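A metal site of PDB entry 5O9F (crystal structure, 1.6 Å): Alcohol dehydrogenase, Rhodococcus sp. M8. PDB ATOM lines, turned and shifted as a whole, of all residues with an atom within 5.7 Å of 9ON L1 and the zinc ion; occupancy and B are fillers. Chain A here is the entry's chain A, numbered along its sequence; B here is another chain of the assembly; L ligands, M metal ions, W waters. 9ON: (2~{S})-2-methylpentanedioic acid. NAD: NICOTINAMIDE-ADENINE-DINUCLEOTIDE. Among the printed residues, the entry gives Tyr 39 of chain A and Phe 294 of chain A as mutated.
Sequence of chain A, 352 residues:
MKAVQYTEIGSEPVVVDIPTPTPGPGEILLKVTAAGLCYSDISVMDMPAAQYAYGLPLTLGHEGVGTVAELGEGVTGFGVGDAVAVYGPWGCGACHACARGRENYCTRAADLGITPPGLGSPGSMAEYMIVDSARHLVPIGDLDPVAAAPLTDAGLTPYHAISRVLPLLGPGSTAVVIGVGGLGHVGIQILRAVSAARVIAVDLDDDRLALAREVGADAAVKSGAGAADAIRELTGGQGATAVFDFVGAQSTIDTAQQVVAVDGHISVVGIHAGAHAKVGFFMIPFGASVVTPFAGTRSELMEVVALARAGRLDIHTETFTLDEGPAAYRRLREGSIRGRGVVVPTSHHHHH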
ATOM      1  N   CYS A  38      13.884  -1.492 -25.423  1.00  0.00           N
ATOM      2  CA  CYS A  38      12.514  -0.925 -25.412  1.00  0.00           C
ATOM      3  C   CYS A  38      12.056  -0.779 -26.858  1.00  0.00           C
ATOM      4  O   CYS A  38      12.838  -0.456 -27.734  1.00  0.00           O
ATOM      5  CB  CYS A  38      12.513   0.442 -24.731  1.00  0.00           C
ATOM      6  SG  CYS A  38      10.888   1.242 -24.702  1.00  0.00           S
ATOM      7  N   TYR A  39      10.761  -1.003 -27.131  1.00  0.00           N
ATOM      8  CA  TYR A  39      10.275  -0.865 -28.502  1.00  0.00           C
ATOM      9  C   TYR A  39      10.473   0.543 -29.056  1.00  0.00           C
ATOM     10  O   TYR A  39      10.621   0.719 -30.277  1.00  0.00           O
ATOM     11  CB  TYR A  39       8.830  -1.365 -28.650  1.00  0.00           C
ATOM     12  CG  TYR A  39       8.454  -1.522 -30.101  1.00  0.00           C
ATOM     13  CD1 TYR A  39       7.905  -0.459 -30.787  1.00  0.00           C
ATOM     14  CD2 TYR A  39       8.711  -2.709 -30.794  1.00  0.00           C
ATOM     15  CE1 TYR A  39       7.572  -0.578 -32.131  1.00  0.00           C
ATOM     16  CE2 TYR A  39       8.390  -2.818 -32.141  1.00  0.00           C
ATOM     17  CZ  TYR A  39       7.833  -1.737 -32.795  1.00  0.00           C
ATOM     18  OH  TYR A  39       7.511  -1.846 -34.120  1.00  0.00           O
ATOM     19  N   SER A  40      10.554   1.543 -28.183  1.00  0.00           N
ATOM     20  CA  SER A  40      10.872   2.889 -28.657  1.00  0.00           C
ATOM     21  C   SER A  40      12.198   2.931 -29.427  1.00  0.00           C
ATOM     22  O   SER A  40      12.354   3.742 -30.327  1.00  0.00           O
ATOM     23  CB  SER A  40      10.934   3.888 -27.498  1.00  0.00           C
ATOM     24  OG  SER A  40       9.677   4.043 -26.861  1.00  0.00           O
ATOM     25  N   ASP A  41      13.144   2.053 -29.076  1.00  0.00           N
ATOM     26  CA  ASP A  41      14.417   1.986 -29.796  1.00  0.00           C
ATOM     27  C   ASP A  41      14.197   1.635 -31.278  1.00  0.00           C
ATOM     28  O   ASP A  41      14.888   2.150 -32.158  1.00  0.00           O
ATOM     29  CB  ASP A  41      15.369   0.960 -29.186  1.00  0.00           C
ATOM     30  CG  ASP A  41      15.785   1.306 -27.771  1.00  0.00           C
ATOM     31  OD1 ASP A  41      15.761   2.521 -27.429  1.00  0.00           O
ATOM     32  OD2 ASP A  41      16.096   0.373 -27.001  1.00  0.00           O
ATOM     33  N   VAL A  44      12.805   4.741 -32.996  1.00  0.00           N
ATOM     34  CA  VAL A  44      13.913   5.680 -33.190  1.00  0.00           C
ATOM     35  C   VAL A  44      14.778   5.288 -34.396  1.00  0.00           C
ATOM     36  O   VAL A  44      15.086   6.133 -35.245  1.00  0.00           O
ATOM     37  CB  VAL A  44      14.774   5.821 -31.916  1.00  0.00           C
ATOM     38  CG1 VAL A  44      16.089   6.537 -32.209  1.00  0.00           C
ATOM     39  CG2 VAL A  44      13.969   6.541 -30.843  1.00  0.00           C
ATOM     40  N   MET A  47      13.259   6.133 -37.826  1.00  0.00           N
ATOM     41  CA  MET A  47      13.142   7.539 -38.240  1.00  0.00           C
ATOM     42  C   MET A  47      14.009   7.812 -39.455  1.00  0.00           C
ATOM     43  O   MET A  47      15.151   7.365 -39.504  1.00  0.00           O
ATOM     44  CB  MET A  47      13.562   8.489 -37.124  1.00  0.00           C
ATOM     45  CG  MET A  47      12.650   8.523 -35.908  1.00  0.00           C
ATOM     46  SD  MET A  47      13.340   9.529 -34.584  1.00  0.00           S
ATOM     47  CE  MET A  47      12.005   9.570 -33.410  1.00  0.00           C
ATOM     48  N   TYR A  54      19.182  12.398 -32.564  1.00  0.00           N
ATOM     49  CA  TYR A  54      19.978  11.956 -31.407  1.00  0.00           C
ATOM     50  C   TYR A  54      21.466  11.801 -31.670  1.00  0.00           C
ATOM     51  O   TYR A  54      22.200  11.458 -30.751  1.00  0.00           O
ATOM     52  CB  TYR A  54      19.404  10.658 -30.847  1.00  0.00           C
ATOM     53  CG  TYR A  54      17.979  10.743 -30.354  1.00  0.00           C
ATOM     54  CD1 TYR A  54      17.432  11.932 -29.861  1.00  0.00           C
ATOM     55  CD2 TYR A  54      17.198   9.607 -30.295  1.00  0.00           C
ATOM     56  CE1 TYR A  54      16.141  11.983 -29.380  1.00  0.00           C
ATOM     57  CE2 TYR A  54      15.909   9.636 -29.793  1.00  0.00           C
ATOM     58  CZ  TYR A  54      15.381  10.831 -29.358  1.00  0.00           C
ATOM     59  OH  TYR A  54      14.096  10.871 -28.864  1.00  0.00           O
ATOM     60  N   HIS A  62      18.148   2.776 -22.887  1.00  0.00           N
ATOM     61  CA  HIS A  62      17.673   3.758 -21.891  1.00  0.00           C
ATOM     62  C   HIS A  62      17.056   3.079 -20.685  1.00  0.00           C
ATOM     63  O   HIS A  62      16.452   3.754 -19.829  1.00  0.00           O
ATOM     64  CB  HIS A  62      16.726   4.814 -22.494  1.00  0.00           C
ATOM     65  CG  HIS A  62      15.545   4.249 -23.205  1.00  0.00           C
ATOM     66  ND1 HIS A  62      15.570   3.874 -24.526  1.00  0.00           N
ATOM     67  CD2 HIS A  62      14.268   4.063 -22.780  1.00  0.00           C
ATOM     68  CE1 HIS A  62      14.362   3.464 -24.890  1.00  0.00           C
ATOM     69  NE2 HIS A  62      13.561   3.562 -23.846  1.00  0.00           N
ATOM     70  N   GLU A  63      17.238   1.762 -20.590  1.00  0.00           N
ATOM     71  CA  GLU A  63      16.928   0.995 -19.390  1.00  0.00           C
ATOM     72  C   GLU A  63      18.227   0.454 -18.833  1.00  0.00           C
ATOM     73  O   GLU A  63      18.731  -0.537 -19.335  1.00  0.00           O
ATOM     74  CB  GLU A  63      15.978  -0.164 -19.732  1.00  0.00           C
ATOM     75  CG  GLU A  63      14.534   0.277 -19.923  1.00  0.00           C
ATOM     76  CD  GLU A  63      13.550  -0.865 -20.121  1.00  0.00           C
ATOM     77  OE1 GLU A  63      13.960  -2.025 -20.364  1.00  0.00           O
ATOM     78  OE2 GLU A  63      12.322  -0.601 -20.036  1.00  0.00           O
ATOM     79  N   LEU A 119      19.263   7.997 -25.835  1.00  0.00           N
ATOM     80  CA  LEU A 119      18.342   8.826 -26.623  1.00  0.00           C
ATOM     81  C   LEU A 119      18.923  10.230 -26.790  1.00  0.00           C
ATOM     82  O   LEU A 119      18.227  11.234 -26.651  1.00  0.00           O
ATOM     83  CB  LEU A 119      16.966   8.854 -25.940  1.00  0.00           C
ATOM     84  CG  LEU A 119      16.214   7.533 -25.785  1.00  0.00           C
ATOM     85  CD1 LEU A 119      15.030   7.664 -24.816  1.00  0.00           C
ATOM     86  CD2 LEU A 119      15.764   6.987 -27.129  1.00  0.00           C
ATOM     87  N   ASP A 153      11.945   1.748 -17.259  1.00  0.00           N
ATOM     88  CA  ASP A 153      11.038   2.300 -18.267  1.00  0.00           C
ATOM     89  C   ASP A 153       9.786   1.429 -18.427  1.00  0.00           C
ATOM     90  O   ASP A 153       8.674   1.934 -18.273  1.00  0.00           O
ATOM     91  CB  ASP A 153      11.774   2.476 -19.586  1.00  0.00           C
ATOM     92  CG  ASP A 153      11.074   3.400 -20.541  1.00  0.00           C
ATOM     93  OD1 ASP A 153      10.228   4.250 -20.147  1.00  0.00           O
ATOM     94  OD2 ASP A 153      11.474   3.297 -21.708  1.00  0.00           O
ATOM     95  N   ILE A 271       3.262   4.583 -28.620  1.00  0.00           N
ATOM     96  CA  ILE A 271       3.580   5.656 -29.561  1.00  0.00           C
ATOM     97  C   ILE A 271       3.517   5.138 -30.992  1.00  0.00           C
ATOM     98  O   ILE A 271       4.391   4.375 -31.452  1.00  0.00           O
ATOM     99  CB  ILE A 271       4.961   6.291 -29.271  1.00  0.00           C
ATOM    100  CG1 ILE A 271       5.028   6.818 -27.825  1.00  0.00           C
ATOM    101  CG2 ILE A 271       5.274   7.399 -30.290  1.00  0.00           C
ATOM    102  CD1 ILE A 271       6.427   7.128 -27.315  1.00  0.00           C
ATOM    103  N   PHE A 294       4.384  10.668 -20.218  1.00  0.00           N
ATOM    104  CA  PHE A 294       5.748  10.421 -20.661  1.00  0.00           C
ATOM    105  C   PHE A 294       6.624  10.015 -19.468  1.00  0.00           C
ATOM    106  O   PHE A 294       6.727  10.779 -18.499  1.00  0.00           O
ATOM    107  CB  PHE A 294       6.334  11.637 -21.338  1.00  0.00           C
ATOM    108  CG  PHE A 294       7.734  11.447 -21.812  1.00  0.00           C
ATOM    109  CD1 PHE A 294       7.986  10.661 -22.949  1.00  0.00           C
ATOM    110  CD2 PHE A 294       8.794  12.011 -21.132  1.00  0.00           C
ATOM    111  CE1 PHE A 294       9.293  10.478 -23.380  1.00  0.00           C
ATOM    112  CE2 PHE A 294      10.104  11.808 -21.564  1.00  0.00           C
ATOM    113  CZ  PHE A 294      10.334  11.049 -22.686  1.00  0.00           C
ATOM    114  N   ARG A 340      10.403  -8.622 -21.704  1.00  0.00           N
ATOM    115  CA  ARG A 340      11.493  -7.699 -21.989  1.00  0.00           C
ATOM    116  C   ARG A 340      12.798  -8.391 -22.347  1.00  0.00           C
ATOM    117  O   ARG A 340      13.235  -9.297 -21.644  1.00  0.00           O
ATOM    118  CB  ARG A 340      11.731  -6.806 -20.761  1.00  0.00           C
ATOM    119  CG  ARG A 340      11.200  -5.403 -20.894  1.00  0.00           C
ATOM    120  CD  ARG A 340      12.057  -4.586 -21.807  1.00  0.00           C
ATOM    121  NE  ARG A 340      11.732  -3.166 -21.715  1.00  0.00           N
ATOM    122  CZ  ARG A 340      10.858  -2.496 -22.463  1.00  0.00           C
ATOM    123  NH1 ARG A 340      10.112  -3.101 -23.381  1.00  0.00           N
ATOM    124  NH2 ARG A 340      10.715  -1.204 -22.267  1.00  0.00           N
ATOM    125  N   PHE B 281       0.649  11.566 -29.532  1.00  0.00           N
ATOM    126  CA  PHE B 281       2.046  11.969 -29.535  1.00  0.00           C
ATOM    127  C   PHE B 281       2.353  12.848 -30.745  1.00  0.00           C
ATOM    128  O   PHE B 281       1.792  12.625 -31.824  1.00  0.00           O
ATOM    129  CB  PHE B 281       2.947  10.753 -29.477  1.00  0.00           C
ATOM    130  CG  PHE B 281       2.932  10.088 -28.120  1.00  0.00           C
ATOM    131  CD1 PHE B 281       3.721  10.590 -27.078  1.00  0.00           C
ATOM    132  CD2 PHE B 281       2.059   9.029 -27.860  1.00  0.00           C
ATOM    133  CE1 PHE B 281       3.660  10.007 -25.815  1.00  0.00           C
ATOM    134  CE2 PHE B 281       2.001   8.457 -26.605  1.00  0.00           C
ATOM    135  CZ  PHE B 281       2.803   8.931 -25.583  1.00  0.00           C
ATOM    136  N   PHE B 282       3.178  13.870 -30.533  1.00  0.00           N
ATOM    137  CA  PHE B 282       3.559  14.847 -31.578  1.00  0.00           C
ATOM    138  C   PHE B 282       2.438  15.856 -31.915  1.00  0.00           C
ATOM    139  O   PHE B 282       2.664  16.739 -32.723  1.00  0.00           O
ATOM    140  CB  PHE B 282       4.044  14.168 -32.884  1.00  0.00           C
ATOM    141  CG  PHE B 282       5.046  13.053 -32.670  1.00  0.00           C
ATOM    142  CD1 PHE B 282       6.373  13.337 -32.360  1.00  0.00           C
ATOM    143  CD2 PHE B 282       4.662  11.709 -32.789  1.00  0.00           C
ATOM    144  CE1 PHE B 282       7.290  12.304 -32.146  1.00  0.00           C
ATOM    145  CE2 PHE B 282       5.573  10.685 -32.588  1.00  0.00           C
ATOM    146  CZ  PHE B 282       6.894  10.989 -32.268  1.00  0.00           C
ATOM    147  N   PHE B 286       3.462  16.467 -23.964  1.00  0.00           N
ATOM    148  CA  PHE B 286       3.480  15.386 -22.970  1.00  0.00           C
ATOM    149  C   PHE B 286       2.718  15.817 -21.727  1.00  0.00           C
ATOM    150  O   PHE B 286       2.869  16.960 -21.233  1.00  0.00           O
ATOM    151  CB  PHE B 286       4.918  15.048 -22.507  1.00  0.00           C
ATOM    152  CG  PHE B 286       5.836  14.490 -23.556  1.00  0.00           C
ATOM    153  CD1 PHE B 286       5.388  13.652 -24.593  1.00  0.00           C
ATOM    154  CD2 PHE B 286       7.199  14.711 -23.452  1.00  0.00           C
ATOM    155  CE1 PHE B 286       6.266  13.131 -25.512  1.00  0.00           C
ATOM    156  CE2 PHE B 286       8.093  14.172 -24.375  1.00  0.00           C
ATOM    157  CZ  PHE B 286       7.631  13.384 -25.414  1.00  0.00           C
HETATM  158  O12 9ON L   1       9.090   9.559 -27.864  1.00  0.00           O
HETATM  159  C7  9ON L   1      10.209   9.402 -27.321  1.00  0.00           C
HETATM  160  O10 9ON L   1      10.727  10.256 -26.564  1.00  0.00           O
HETATM  161  C4  9ON L   1      10.974   8.145 -27.638  1.00  0.00           C
HETATM  162  C5  9ON L   1      12.051   8.490 -28.662  1.00  0.00           C
HETATM  163  C3  9ON L   1      11.578   7.524 -26.377  1.00  0.00           C
HETATM  164  C2  9ON L   1      10.504   7.031 -25.403  1.00  0.00           C
HETATM  165  C1  9ON L   1      11.120   6.085 -24.393  1.00  0.00           C
HETATM  166  O8  9ON L   1      11.776   6.609 -23.466  1.00  0.00           O
HETATM  167  O9  9ON L   1      10.940   4.843 -24.505  1.00  0.00           O
HETATM  168  PA  NAD L   2       6.623  -4.532 -27.013  1.00  0.00           P
HETATM  169  O1A NAD L   2       6.965  -4.702 -28.482  1.00  0.00           O
HETATM  170  O2A NAD L   2       7.370  -5.219 -25.901  1.00  0.00           O
HETATM  171  O5B NAD L   2       5.098  -4.996 -26.766  1.00  0.00           O
HETATM  172  C5B NAD L   2       4.065  -4.832 -27.741  1.00  0.00           C
HETATM  173  C4B NAD L   2       2.861  -5.627 -27.284  1.00  0.00           C
HETATM  174  O4B NAD L   2       1.716  -5.036 -27.902  1.00  0.00           O
HETATM  175  C3B NAD L   2       2.913  -7.084 -27.732  1.00  0.00           C
HETATM  176  O3B NAD L   2       2.446  -7.968 -26.710  1.00  0.00           O
HETATM  177  C2B NAD L   2       2.011  -7.103 -28.945  1.00  0.00           C
HETATM  178  O2B NAD L   2       1.396  -8.338 -29.265  1.00  0.00           O
HETATM  179  C1B NAD L   2       0.974  -6.072 -28.539  1.00  0.00           C
HETATM  180  N9A NAD L   2       0.208  -5.460 -29.625  1.00  0.00           N
HETATM  181  C8A NAD L   2       0.683  -4.921 -30.764  1.00  0.00           C
HETATM  182  N7A NAD L   2      -0.331  -4.418 -31.505  1.00  0.00           N
HETATM  183  C5A NAD L   2      -1.467  -4.616 -30.813  1.00  0.00           C
HETATM  184  C6A NAD L   2      -2.900  -4.327 -30.983  1.00  0.00           C
HETATM  185  N6A NAD L   2      -3.351  -3.708 -32.105  1.00  0.00           N
HETATM  186  N1A NAD L   2      -3.754  -4.684 -30.012  1.00  0.00           N
HETATM  187  C2A NAD L   2      -3.346  -5.317 -28.892  1.00  0.00           C
HETATM  188  N3A NAD L   2      -2.057  -5.626 -28.664  1.00  0.00           N
HETATM  189  C4A NAD L   2      -1.103  -5.303 -29.563  1.00  0.00           C
HETATM  190  O3  NAD L   2       6.544  -2.947 -26.723  1.00  0.00           O
HETATM  191  PN  NAD L   2       7.007  -2.127 -25.395  1.00  0.00           P
HETATM  192  O1N NAD L   2       8.490  -1.986 -25.396  1.00  0.00           O
HETATM  193  O2N NAD L   2       6.208  -2.681 -24.248  1.00  0.00           O
HETATM  194  O5D NAD L   2       6.481  -0.672 -25.862  1.00  0.00           O
HETATM  195  C5D NAD L   2       5.082  -0.422 -25.985  1.00  0.00           C
HETATM  196  C4D NAD L   2       4.860   0.962 -26.560  1.00  0.00           C
HETATM  197  O4D NAD L   2       5.110   1.919 -25.511  1.00  0.00           O
HETATM  198  C3D NAD L   2       5.738   1.365 -27.729  1.00  0.00           C
HETATM  199  O3D NAD L   2       4.999   2.183 -28.661  1.00  0.00           O
HETATM  200  C2D NAD L   2       6.800   2.225 -27.091  1.00  0.00           C
HETATM  201  O2D NAD L   2       7.436   3.128 -27.986  1.00  0.00           O
HETATM  202  C1D NAD L   2       5.951   2.942 -26.042  1.00  0.00           C
HETATM  203  N1N NAD L   2       6.644   3.557 -24.902  1.00  0.00           N
HETATM  204  C2N NAD L   2       6.194   4.740 -24.461  1.00  0.00           C
HETATM  205  C3N NAD L   2       6.727   5.391 -23.367  1.00  0.00           C
HETATM  206  C7N NAD L   2       6.189   6.714 -22.910  1.00  0.00           C
HETATM  207  O7N NAD L   2       6.865   7.393 -22.147  1.00  0.00           O
HETATM  208  N7N NAD L   2       4.937   7.084 -23.236  1.00  0.00           N
HETATM  209  C4N NAD L   2       7.807   4.799 -22.693  1.00  0.00           C
HETATM  210  C5N NAD L   2       8.212   3.530 -23.123  1.00  0.00           C
HETATM  211  C6N NAD L   2       7.634   2.925 -24.224  1.00  0.00           C
HETATM  212 ZN    ZN M   1      11.585   3.205 -23.666  1.00  0.00          ZN
HETATM  213  O   HOH W   1      11.296  13.007 -25.922  1.00  0.00           O
HETATM  214  O   HOH W   2      13.203  11.159 -24.859  1.00  0.00           O
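Ser 40 touches the zinc ion.
Of the 17 residues printed, 4 come within 4 Å of the zinc ion.
Residues that only touch 9ON L1: Val 44 (3.5 Å), Tyr 54 (3.1 Å), Leu 119 (3.7 Å), Ile 271 (3.6 Å) and Phe 294 (3.5 Å).
N of Cys 38 lies within hydrogen-bond range of OD2 of Asp 41.
The side-chain carboxylate of Asp 41 lies close to a ring nitrogen (ND1) of His 62, 3.2 Å away.
The guanidinium group of Arg 340 lies close to the side-chain sulfur of Cys 38.
The side-chain sulfur (SG) of Cys 38 lies close to the backbone NH (N) of Ser 40 (3.5 Å).
NH1 of Arg 340 is in salt-bridge range of O1N of NAD L2.
OG of Ser 40 is in hydrogen-bond range of O2D of NAD L2 (2.7 Å).
The side-chain hydroxyl of Ser 40 lies close to an oxygen (O9) of 9ON L1 (2.8 Å).
O3D of NAD L2 is in hydrogen-bond range of N of Ile 271, 3.0 Å away.
N of Tyr 39 lies within hydrogen-bond range of O1N of NAD L2 (3.0 Å).
The zinc ion is bound by O9 of 9ON L1 (2.0 Å), OD2 of Asp 153 (2.0 Å), NE2 of His 62 (2.0 Å) and SG of Cys 38 (2.3 Å).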
